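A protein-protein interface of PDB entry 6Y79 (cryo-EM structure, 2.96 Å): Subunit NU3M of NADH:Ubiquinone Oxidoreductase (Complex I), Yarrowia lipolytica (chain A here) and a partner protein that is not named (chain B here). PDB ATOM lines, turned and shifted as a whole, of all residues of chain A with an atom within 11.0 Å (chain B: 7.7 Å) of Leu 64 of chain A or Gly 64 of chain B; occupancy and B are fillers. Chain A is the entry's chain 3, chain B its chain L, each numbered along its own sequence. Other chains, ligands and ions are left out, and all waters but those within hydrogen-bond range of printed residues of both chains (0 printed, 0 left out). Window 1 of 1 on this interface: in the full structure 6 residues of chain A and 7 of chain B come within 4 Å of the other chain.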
ATOM      1  N   PHE A  56      30.211 -16.427 -11.333  1.00  0.00           N
ATOM      2  CA  PHE A  56      30.134 -15.634 -10.105  1.00  0.00           C
ATOM      3  C   PHE A  56      29.505 -14.288 -10.350  1.00  0.00           C
ATOM      4  O   PHE A  56      28.685 -13.811  -9.563  1.00  0.00           O
ATOM      5  CB  PHE A  56      31.513 -15.359  -9.540  1.00  0.00           C
ATOM      6  CG  PHE A  56      32.212 -16.537  -9.102  1.00  0.00           C
ATOM      7  CD1 PHE A  56      31.943 -17.076  -7.873  1.00  0.00           C
ATOM      8  CD2 PHE A  56      33.144 -17.114  -9.910  1.00  0.00           C
ATOM      9  CE1 PHE A  56      32.602 -18.183  -7.444  1.00  0.00           C
ATOM     10  CE2 PHE A  56      33.820 -18.221  -9.504  1.00  0.00           C
ATOM     11  CZ  PHE A  56      33.537 -18.726  -8.278  1.00  0.00           C
ATOM     12  N   ILE A  57      29.976 -13.606 -11.379  1.00  0.00           N
ATOM     13  CA  ILE A  57      29.433 -12.295 -11.647  1.00  0.00           C
ATOM     14  C   ILE A  57      28.084 -12.457 -12.315  1.00  0.00           C
ATOM     15  O   ILE A  57      27.180 -11.634 -12.119  1.00  0.00           O
ATOM     16  CB  ILE A  57      30.456 -11.483 -12.464  1.00  0.00           C
ATOM     17  CG1 ILE A  57      30.094 -10.021 -12.423  1.00  0.00           C
ATOM     18  CG2 ILE A  57      30.659 -12.015 -13.882  1.00  0.00           C
ATOM     19  CD1 ILE A  57      30.434  -9.449 -11.109  1.00  0.00           C
ATOM     20  N   LEU A  58      27.897 -13.584 -13.004  1.00  0.00           N
ATOM     21  CA  LEU A  58      26.668 -13.838 -13.724  1.00  0.00           C
ATOM     22  C   LEU A  58      25.488 -14.063 -12.791  1.00  0.00           C
ATOM     23  O   LEU A  58      24.396 -13.598 -13.107  1.00  0.00           O
ATOM     24  CB  LEU A  58      26.865 -15.036 -14.644  1.00  0.00           C
ATOM     25  CG  LEU A  58      25.762 -15.324 -15.644  1.00  0.00           C
ATOM     26  CD1 LEU A  58      25.699 -14.237 -16.696  1.00  0.00           C
ATOM     27  CD2 LEU A  58      26.031 -16.655 -16.265  1.00  0.00           C
ATOM     28  N   VAL A  59      25.677 -14.748 -11.648  1.00  0.00           N
ATOM     29  CA  VAL A  59      24.543 -15.061 -10.768  1.00  0.00           C
ATOM     30  C   VAL A  59      23.915 -13.784 -10.213  1.00  0.00           C
ATOM     31  O   VAL A  59      22.693 -13.616 -10.247  1.00  0.00           O
ATOM     32  CB  VAL A  59      24.950 -16.055  -9.654  1.00  0.00           C
ATOM     33  CG1 VAL A  59      26.114 -15.586  -8.820  1.00  0.00           C
ATOM     34  CG2 VAL A  59      23.781 -16.352  -8.736  1.00  0.00           C
ATOM     35  N   ALA A  60      24.737 -12.807  -9.853  1.00  0.00           N
ATOM     36  CA  ALA A  60      24.202 -11.559  -9.338  1.00  0.00           C
ATOM     37  C   ALA A  60      23.821 -10.566 -10.419  1.00  0.00           C
ATOM     38  O   ALA A  60      23.017  -9.670 -10.145  1.00  0.00           O
ATOM     39  CB  ALA A  60      25.200 -10.895  -8.397  1.00  0.00           C
ATOM     40  N   ILE A  61      24.370 -10.667 -11.633  1.00  0.00           N
ATOM     41  CA  ILE A  61      23.842  -9.796 -12.677  1.00  0.00           C
ATOM     42  C   ILE A  61      22.491 -10.307 -13.159  1.00  0.00           C
ATOM     43  O   ILE A  61      21.514  -9.553 -13.192  1.00  0.00           O
ATOM     44  CB  ILE A  61      24.835  -9.620 -13.838  1.00  0.00           C
ATOM     45  CG1 ILE A  61      26.071  -8.860 -13.378  1.00  0.00           C
ATOM     46  CG2 ILE A  61      24.211  -8.773 -14.888  1.00  0.00           C
ATOM     47  CD1 ILE A  61      27.155  -8.768 -14.426  1.00  0.00           C
ATOM     48  N   LEU A  62      22.385 -11.599 -13.496  1.00  0.00           N
ATOM     49  CA  LEU A  62      21.087 -12.099 -13.937  1.00  0.00           C
ATOM     50  C   LEU A  62      20.114 -12.288 -12.788  1.00  0.00           C
ATOM     51  O   LEU A  62      18.976 -12.672 -13.042  1.00  0.00           O
ATOM     52  CB  LEU A  62      21.180 -13.420 -14.725  1.00  0.00           C
ATOM     53  CG  LEU A  62      21.629 -14.801 -14.219  1.00  0.00           C
ATOM     54  CD1 LEU A  62      20.599 -15.597 -13.426  1.00  0.00           C
ATOM     55  CD2 LEU A  62      22.032 -15.629 -15.416  1.00  0.00           C
ATOM     56  N   PHE A  63      20.538 -12.096 -11.536  1.00  0.00           N
ATOM     57  CA  PHE A  63      19.597 -12.133 -10.425  1.00  0.00           C
ATOM     58  C   PHE A  63      18.536 -11.056 -10.548  1.00  0.00           C
ATOM     59  O   PHE A  63      17.351 -11.310 -10.311  1.00  0.00           O
ATOM     60  CB  PHE A  63      20.335 -11.959  -9.104  1.00  0.00           C
ATOM     61  CG  PHE A  63      19.416 -11.795  -7.949  1.00  0.00           C
ATOM     62  CD1 PHE A  63      18.652 -12.859  -7.541  1.00  0.00           C
ATOM     63  CD2 PHE A  63      19.274 -10.576  -7.297  1.00  0.00           C
ATOM     64  CE1 PHE A  63      17.784 -12.724  -6.507  1.00  0.00           C
ATOM     65  CE2 PHE A  63      18.393 -10.447  -6.249  1.00  0.00           C
ATOM     66  CZ  PHE A  63      17.651 -11.527  -5.860  1.00  0.00           C
ATOM     67  N   LEU A  64      18.942  -9.861 -10.901  1.00  0.00           N
ATOM     68  CA  LEU A  64      18.106  -8.669 -10.909  1.00  0.00           C
ATOM     69  C   LEU A  64      16.933  -8.693 -11.903  1.00  0.00           C
ATOM     70  O   LEU A  64      15.857  -8.209 -11.534  1.00  0.00           O
ATOM     71  CB  LEU A  64      19.016  -7.454 -11.125  1.00  0.00           C
ATOM     72  CG  LEU A  64      18.532  -6.047 -10.824  1.00  0.00           C
ATOM     73  CD1 LEU A  64      19.676  -5.213 -10.315  1.00  0.00           C
ATOM     74  CD2 LEU A  64      18.025  -5.462 -12.086  1.00  0.00           C
ATOM     75  N   PRO A  65      17.050  -9.196 -13.149  1.00  0.00           N
ATOM     76  CA  PRO A  65      15.845  -9.275 -13.989  1.00  0.00           C
ATOM     77  C   PRO A  65      14.803 -10.270 -13.516  1.00  0.00           C
ATOM     78  O   PRO A  65      13.635 -10.120 -13.884  1.00  0.00           O
ATOM     79  CB  PRO A  65      16.401  -9.678 -15.357  1.00  0.00           C
ATOM     80  CG  PRO A  65      17.728  -9.130 -15.359  1.00  0.00           C
ATOM     81  CD  PRO A  65      18.235  -9.414 -14.004  1.00  0.00           C
ATOM     82  N   PHE A  66      15.169 -11.284 -12.733  1.00  0.00           N
ATOM     83  CA  PHE A  66      14.141 -12.151 -12.170  1.00  0.00           C
ATOM     84  C   PHE A  66      13.483 -11.493 -10.966  1.00  0.00           C
ATOM     85  O   PHE A  66      12.268 -11.607 -10.780  1.00  0.00           O
ATOM     86  CB  PHE A  66      14.729 -13.507 -11.787  1.00  0.00           C
ATOM     87  CG  PHE A  66      15.151 -14.350 -12.957  1.00  0.00           C
ATOM     88  CD1 PHE A  66      14.229 -15.087 -13.681  1.00  0.00           C
ATOM     89  CD2 PHE A  66      16.476 -14.430 -13.314  1.00  0.00           C
ATOM     90  CE1 PHE A  66      14.639 -15.872 -14.753  1.00  0.00           C
ATOM     91  CE2 PHE A  66      16.891 -15.209 -14.380  1.00  0.00           C
ATOM     92  CZ  PHE A  66      15.975 -15.927 -15.096  1.00  0.00           C
ATOM     93  N   ASP A  67      14.275 -10.777 -10.166  1.00  0.00           N
ATOM     94  CA  ASP A  67      13.757 -10.019  -9.031  1.00  0.00           C
ATOM     95  C   ASP A  67      12.793  -8.925  -9.473  1.00  0.00           C
ATOM     96  O   ASP A  67      11.792  -8.663  -8.797  1.00  0.00           O
ATOM     97  CB  ASP A  67      14.927  -9.410  -8.261  1.00  0.00           C
ATOM     98  CG  ASP A  67      14.516  -8.797  -6.945  1.00  0.00           C
ATOM     99  OD1 ASP A  67      13.406  -9.077  -6.455  1.00  0.00           O
ATOM    100  OD2 ASP A  67      15.317  -8.018  -6.393  1.00  0.00           O
ATOM    101  N   LEU A  68      13.078  -8.269 -10.600  1.00  0.00           N
ATOM    102  CA  LEU A  68      12.162  -7.256 -11.108  1.00  0.00           C
ATOM    103  C   LEU A  68      10.877  -7.871 -11.639  1.00  0.00           C
ATOM    104  O   LEU A  68       9.844  -7.202 -11.654  1.00  0.00           O
ATOM    105  CB  LEU A  68      12.829  -6.430 -12.203  1.00  0.00           C
ATOM    106  CG  LEU A  68      13.931  -5.464 -11.796  1.00  0.00           C
ATOM    107  CD1 LEU A  68      14.487  -4.828 -13.032  1.00  0.00           C
ATOM    108  CD2 LEU A  68      13.404  -4.412 -10.857  1.00  0.00           C
ATOM    109  N   GLU A  69      10.915  -9.130 -12.082  1.00  0.00           N
ATOM    110  CA  GLU A  69       9.681  -9.811 -12.458  1.00  0.00           C
ATOM    111  C   GLU A  69       8.857 -10.160 -11.229  1.00  0.00           C
ATOM    112  O   GLU A  69       7.630  -9.989 -11.227  1.00  0.00           O
ATOM    113  CB  GLU A  69       9.954 -11.079 -13.264  1.00  0.00           C
ATOM    114  CG  GLU A  69       8.620 -11.736 -13.607  1.00  0.00           C
ATOM    115  CD  GLU A  69       8.699 -13.221 -13.924  1.00  0.00           C
ATOM    116  OE1 GLU A  69       9.248 -13.949 -13.088  1.00  0.00           O
ATOM    117  OE2 GLU A  69       8.113 -13.617 -14.948  1.00  0.00           O
ATOM    118  N   ILE A  70       9.516 -10.652 -10.172  1.00  0.00           N
ATOM    119  CA  ILE A  70       8.801 -11.069  -8.967  1.00  0.00           C
ATOM    120  C   ILE A  70       8.081  -9.889  -8.315  1.00  0.00           C
ATOM    121  O   ILE A  70       6.945 -10.030  -7.857  1.00  0.00           O
ATOM    122  CB  ILE A  70       9.762 -11.780  -7.987  1.00  0.00           C
ATOM    123  CG1 ILE A  70      10.399 -13.007  -8.629  1.00  0.00           C
ATOM    124  CG2 ILE A  70       9.038 -12.293  -6.792  1.00  0.00           C
ATOM    125  CD1 ILE A  70       9.419 -14.004  -9.159  1.00  0.00           C
ATOM    126  N   SER A  71       8.667  -8.696  -8.345  1.00  0.00           N
ATOM    127  CA  SER A  71       7.925  -7.538  -7.862  1.00  0.00           C
ATOM    128  C   SER A  71       7.021  -6.912  -8.921  1.00  0.00           C
ATOM    129  O   SER A  71       6.346  -5.925  -8.621  1.00  0.00           O
ATOM    130  CB  SER A  71       8.877  -6.475  -7.314  1.00  0.00           C
ATOM    131  OG  SER A  71       9.645  -5.892  -8.346  1.00  0.00           O
ATOM    132  N   THR A  72       7.002  -7.438 -10.145  1.00  0.00           N
ATOM    133  CA  THR A  72       5.998  -7.052 -11.132  1.00  0.00           C
ATOM    134  C   THR A  72       4.730  -7.891 -11.001  1.00  0.00           C
ATOM    135  O   THR A  72       3.642  -7.433 -11.369  1.00  0.00           O
ATOM    136  CB  THR A  72       6.588  -7.162 -12.551  1.00  0.00           C
ATOM    137  OG1 THR A  72       7.873  -6.536 -12.574  1.00  0.00           O
ATOM    138  CG2 THR A  72       5.726  -6.465 -13.587  1.00  0.00           C
ATOM    139  N   PHE A  94       2.685 -12.657 -19.935  1.00  0.00           N
ATOM    140  CA  PHE A  94       3.866 -12.059 -19.304  1.00  0.00           C
ATOM    141  C   PHE A  94       4.799 -13.123 -18.733  1.00  0.00           C
ATOM    142  O   PHE A  94       6.008 -13.147 -19.028  1.00  0.00           O
ATOM    143  CB  PHE A  94       3.389 -11.099 -18.209  1.00  0.00           C
ATOM    144  CG  PHE A  94       4.485 -10.421 -17.447  1.00  0.00           C
ATOM    145  CD1 PHE A  94       5.146  -9.356 -17.997  1.00  0.00           C
ATOM    146  CD2 PHE A  94       4.789 -10.786 -16.148  1.00  0.00           C
ATOM    147  CE1 PHE A  94       6.163  -8.713 -17.310  1.00  0.00           C
ATOM    148  CE2 PHE A  94       5.784 -10.139 -15.452  1.00  0.00           C
ATOM    149  CZ  PHE A  94       6.470  -9.100 -16.036  1.00  0.00           C
ATOM    150  N   LEU A  98       8.632 -14.488 -20.051  1.00  0.00           N
ATOM    151  CA  LEU A  98       9.845 -14.568 -19.240  1.00  0.00           C
ATOM    152  C   LEU A  98      10.331 -16.005 -19.007  1.00  0.00           C
ATOM    153  O   LEU A  98      11.532 -16.230 -18.791  1.00  0.00           O
ATOM    154  CB  LEU A  98       9.602 -13.807 -17.954  1.00  0.00           C
ATOM    155  CG  LEU A  98       9.505 -12.370 -18.453  1.00  0.00           C
ATOM    156  CD1 LEU A  98       8.579 -11.557 -17.607  1.00  0.00           C
ATOM    157  CD2 LEU A  98      10.881 -11.776 -18.468  1.00  0.00           C
ATOM    158  N   GLU A 105      18.296 -19.404 -20.727  1.00  0.00           N
ATOM    159  CA  GLU A 105      19.378 -19.396 -19.742  1.00  0.00           C
ATOM    160  C   GLU A 105      19.795 -20.805 -19.327  1.00  0.00           C
ATOM    161  O   GLU A 105      20.985 -21.081 -19.156  1.00  0.00           O
ATOM    162  CB  GLU A 105      18.950 -18.593 -18.515  1.00  0.00           C
ATOM    163  CG  GLU A 105      20.068 -18.326 -17.538  1.00  0.00           C
ATOM    164  CD  GLU A 105      20.119 -19.321 -16.408  1.00  0.00           C
ATOM    165  OE1 GLU A 105      19.048 -19.811 -16.006  1.00  0.00           O
ATOM    166  OE2 GLU A 105      21.234 -19.629 -15.935  1.00  0.00           O
ATOM    167  N   LEU A 111      25.066 -20.637 -15.794  1.00  0.00           N
ATOM    168  CA  LEU A 111      25.492 -20.427 -14.417  1.00  0.00           C
ATOM    169  C   LEU A 111      26.459 -21.484 -13.905  1.00  0.00           C
ATOM    170  O   LEU A 111      26.783 -21.478 -12.715  1.00  0.00           O
ATOM    171  CB  LEU A 111      24.269 -20.362 -13.509  1.00  0.00           C
ATOM    172  CG  LEU A 111      23.602 -18.997 -13.569  1.00  0.00           C
ATOM    173  CD1 LEU A 111      22.336 -18.987 -12.767  1.00  0.00           C
ATOM    174  CD2 LEU A 111      24.564 -17.968 -13.057  1.00  0.00           C
ATOM    175  N   GLU B  30      21.980   6.781 -11.255  1.00  0.00           N
ATOM    176  CA  GLU B  30      20.862   6.214 -10.500  1.00  0.00           C
ATOM    177  C   GLU B  30      20.180   7.256  -9.618  1.00  0.00           C
ATOM    178  O   GLU B  30      18.950   7.246  -9.471  1.00  0.00           O
ATOM    179  CB  GLU B  30      21.340   5.036  -9.663  1.00  0.00           C
ATOM    180  CG  GLU B  30      21.853   3.888 -10.495  1.00  0.00           C
ATOM    181  CD  GLU B  30      20.802   3.316 -11.426  1.00  0.00           C
ATOM    182  OE1 GLU B  30      19.642   3.138 -10.999  1.00  0.00           O
ATOM    183  OE2 GLU B  30      21.137   3.030 -12.595  1.00  0.00           O
ATOM    184  N   LEU B  33      17.827   9.281 -11.719  1.00  0.00           N
ATOM    185  CA  LEU B  33      16.556   8.572 -11.889  1.00  0.00           C
ATOM    186  C   LEU B  33      15.676   8.662 -10.644  1.00  0.00           C
ATOM    187  O   LEU B  33      14.446   8.775 -10.749  1.00  0.00           O
ATOM    188  CB  LEU B  33      16.823   7.115 -12.237  1.00  0.00           C
ATOM    189  CG  LEU B  33      17.360   6.931 -13.643  1.00  0.00           C
ATOM    190  CD1 LEU B  33      18.111   5.625 -13.750  1.00  0.00           C
ATOM    191  CD2 LEU B  33      16.208   6.990 -14.618  1.00  0.00           C
ATOM    192  N   VAL B  58       6.908   1.966 -13.933  1.00  0.00           N
ATOM    193  CA  VAL B  58       7.578   1.435 -15.114  1.00  0.00           C
ATOM    194  C   VAL B  58       9.039   1.882 -15.165  1.00  0.00           C
ATOM    195  O   VAL B  58       9.941   1.095 -15.495  1.00  0.00           O
ATOM    196  CB  VAL B  58       6.782   1.842 -16.364  1.00  0.00           C
ATOM    197  CG1 VAL B  58       7.557   1.575 -17.600  1.00  0.00           C
ATOM    198  CG2 VAL B  58       5.485   1.062 -16.411  1.00  0.00           C
ATOM    199  N   ILE B  59       9.312   3.129 -14.783  1.00  0.00           N
ATOM    200  CA  ILE B  59      10.682   3.620 -14.818  1.00  0.00           C
ATOM    201  C   ILE B  59      11.541   3.052 -13.684  1.00  0.00           C
ATOM    202  O   ILE B  59      12.768   3.023 -13.820  1.00  0.00           O
ATOM    203  CB  ILE B  59      10.646   5.160 -14.846  1.00  0.00           C
ATOM    204  CG1 ILE B  59      11.956   5.761 -15.336  1.00  0.00           C
ATOM    205  CG2 ILE B  59      10.368   5.702 -13.522  1.00  0.00           C
ATOM    206  CD1 ILE B  59      11.891   7.255 -15.484  1.00  0.00           C
ATOM    207  N   ILE B  60      10.932   2.541 -12.603  1.00  0.00           N
ATOM    208  CA  ILE B  60      11.679   1.759 -11.608  1.00  0.00           C
ATOM    209  C   ILE B  60      12.298   0.525 -12.253  1.00  0.00           C
ATOM    210  O   ILE B  60      13.498   0.246 -12.106  1.00  0.00           O
ATOM    211  CB  ILE B  60      10.758   1.365 -10.437  1.00  0.00           C
ATOM    212  CG1 ILE B  60      10.507   2.545  -9.500  1.00  0.00           C
ATOM    213  CG2 ILE B  60      11.327   0.198  -9.644  1.00  0.00           C
ATOM    214  CD1 ILE B  60       9.388   2.302  -8.515  1.00  0.00           C
ATOM    215  N   ILE B  61      11.486  -0.208 -13.010  1.00  0.00           N
ATOM    216  CA  ILE B  61      11.915  -1.436 -13.664  1.00  0.00           C
ATOM    217  C   ILE B  61      12.942  -1.143 -14.745  1.00  0.00           C
ATOM    218  O   ILE B  61      13.940  -1.864 -14.889  1.00  0.00           O
ATOM    219  CB  ILE B  61      10.677  -2.153 -14.223  1.00  0.00           C
ATOM    220  CG1 ILE B  61       9.770  -2.600 -13.085  1.00  0.00           C
ATOM    221  CG2 ILE B  61      11.057  -3.308 -15.043  1.00  0.00           C
ATOM    222  CD1 ILE B  61       8.433  -3.059 -13.550  1.00  0.00           C
ATOM    223  N   LEU B  62      12.735  -0.062 -15.499  1.00  0.00           N
ATOM    224  CA  LEU B  62      13.694   0.307 -16.535  1.00  0.00           C
ATOM    225  C   LEU B  62      15.029   0.755 -15.948  1.00  0.00           C
ATOM    226  O   LEU B  62      16.081   0.455 -16.523  1.00  0.00           O
ATOM    227  CB  LEU B  62      13.095   1.388 -17.429  1.00  0.00           C
ATOM    228  CG  LEU B  62      11.935   0.865 -18.278  1.00  0.00           C
ATOM    229  CD1 LEU B  62      11.288   1.959 -19.061  1.00  0.00           C
ATOM    230  CD2 LEU B  62      12.411  -0.186 -19.215  1.00  0.00           C
ATOM    231  N   ALA B  63      15.014   1.426 -14.790  1.00  0.00           N
ATOM    232  CA  ALA B  63      16.257   1.779 -14.109  1.00  0.00           C
ATOM    233  C   ALA B  63      17.005   0.543 -13.632  1.00  0.00           C
ATOM    234  O   ALA B  63      18.238   0.471 -13.748  1.00  0.00           O
ATOM    235  CB  ALA B  63      15.960   2.698 -12.927  1.00  0.00           C
ATOM    236  N   GLY B  64      16.273  -0.442 -13.107  1.00  0.00           N
ATOM    237  CA  GLY B  64      16.904  -1.693 -12.712  1.00  0.00           C
ATOM    238  C   GLY B  64      17.553  -2.425 -13.873  1.00  0.00           C
ATOM    239  O   GLY B  64      18.713  -2.845 -13.788  1.00  0.00           O
ATOM    240  N   VAL B  65      16.825  -2.549 -14.989  1.00  0.00           N
ATOM    241  CA  VAL B  65      17.353  -3.238 -16.166  1.00  0.00           C
ATOM    242  C   VAL B  65      18.549  -2.495 -16.750  1.00  0.00           C
ATOM    243  O   VAL B  65      19.521  -3.129 -17.174  1.00  0.00           O
ATOM    244  CB  VAL B  65      16.235  -3.452 -17.208  1.00  0.00           C
ATOM    245  CG1 VAL B  65      16.768  -4.062 -18.497  1.00  0.00           C
ATOM    246  CG2 VAL B  65      15.185  -4.371 -16.651  1.00  0.00           C
ATOM    247  N   GLU B  66      18.548  -1.156 -16.714  1.00  0.00           N
ATOM    248  CA  GLU B  66      19.703  -0.421 -17.222  1.00  0.00           C
ATOM    249  C   GLU B  66      20.921  -0.614 -16.328  1.00  0.00           C
ATOM    250  O   GLU B  66      22.048  -0.714 -16.826  1.00  0.00           O
ATOM    251  CB  GLU B  66      19.394   1.070 -17.380  1.00  0.00           C
ATOM    252  CG  GLU B  66      20.524   1.764 -18.130  1.00  0.00           C
ATOM    253  CD  GLU B  66      20.323   3.225 -18.464  1.00  0.00           C
ATOM    254  OE1 GLU B  66      19.241   3.776 -18.189  1.00  0.00           O
ATOM    255  OE2 GLU B  66      21.281   3.830 -18.991  1.00  0.00           O
ATOM    256  N   SER B  67      20.711  -0.719 -15.010  1.00  0.00           N
ATOM    257  CA  SER B  67      21.820  -1.017 -14.104  1.00  0.00           C
ATOM    258  C   SER B  67      22.417  -2.393 -14.372  1.00  0.00           C
ATOM    259  O   SER B  67      23.641  -2.550 -14.405  1.00  0.00           O
ATOM    260  CB  SER B  67      21.356  -0.912 -12.659  1.00  0.00           C
ATOM    261  OG  SER B  67      20.849   0.378 -12.395  1.00  0.00           O
ATOM    262  N   ALA B  68      21.565  -3.391 -14.611  1.00  0.00           N
ATOM    263  CA  ALA B  68      22.055  -4.737 -14.918  1.00  0.00           C
ATOM    264  C   ALA B  68      22.837  -4.767 -16.230  1.00  0.00           C
ATOM    265  O   ALA B  68      23.958  -5.306 -16.286  1.00  0.00           O
ATOM    266  CB  ALA B  68      20.881  -5.711 -14.969  1.00  0.00           C
ATOM    267  N   ILE B  69      22.268  -4.156 -17.282  1.00  0.00           N
ATOM    268  CA  ILE B  69      22.902  -4.090 -18.603  1.00  0.00           C
ATOM    269  C   ILE B  69      24.250  -3.389 -18.518  1.00  0.00           C
ATOM    270  O   ILE B  69      25.279  -3.926 -18.941  1.00  0.00           O
ATOM    271  CB  ILE B  69      21.983  -3.377 -19.614  1.00  0.00           C
ATOM    272  CG1 ILE B  69      20.738  -4.193 -19.948  1.00  0.00           C
ATOM    273  CG2 ILE B  69      22.730  -3.066 -20.896  1.00  0.00           C
ATOM    274  CD1 ILE B  69      21.006  -5.502 -20.567  1.00  0.00           C
ATOM    275  N   GLY B  70      24.268  -2.189 -17.940  1.00  0.00           N
ATOM    276  CA  GLY B  70      25.477  -1.395 -17.892  1.00  0.00           C
ATOM    277  C   GLY B  70      26.551  -1.937 -16.987  1.00  0.00           C
ATOM    278  O   GLY B  70      27.737  -1.720 -17.253  1.00  0.00           O
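Among the printed residues, pairs that only touch across the chains: Ile 61 of chain A with Ala 68 of chain B (3.7 Å), Leu 64 of chain A with Gly 64 of chain B (3.2 Å), Leu 68 of chain A with Ile 61 of chain B (3.5 Å), Leu 68 of chain A with Gly 64 of chain B (3.97 Å), Leu 68 of chain A with Val 65 of chain B (3.7 Å) and Thr 72 of chain A with Ile 61 of chain B (3.7 Å).
Of the 21 printed residues of chain A, 4 touch a printed residue of chain B. Hydrophobic or aromatic side chains of chain A within 4 Å of the printed part of chain B: Ile 61, Leu 64 and Leu 68. Of the 15 printed residues of chain B, 4 touch a printed residue of chain A. Along chain B the printed residues that touch a printed residue of chain A span positions 61 to 68. Among the printed residues, 6 pairs touch across the chains. Among the printed residues, no Asp or Glu carboxylate lies within 4 Å of a Lys or Arg side-chain nitrogen of the other chain.
Leu 64 of chain A touches one residue of chain B. Of chain A, only Leu 64 (3.2 Å) and Leu 68 (3.97 Å) come within 4 Å of Gly 64 of chain B. No residue of chain A comes within 4 Å of Ala 63 of chain B. No residue of chain A comes within 4 Å of Ser 67 of chain B. Ala 68 of chain B touches just one residue of chain A: Ile 61 (3.7 Å). Printed residues of chain A within 4 Å of Ile 61 of chain B: Leu 68 (3.5 Å) and Thr 72 (3.7 Å). Printed residues of chain B within 4 Å of Leu 68 of chain A: Ile 61, Gly 64 and Val 65. Phe 63 of chain A touches none of the printed residues of chain B. Leu 62 of chain A touches none of the printed residues of chain B. The nearest printed residue of chain B that does not touch Ile 61 of chain A is Ile 69 of chain B (5.6 Å).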
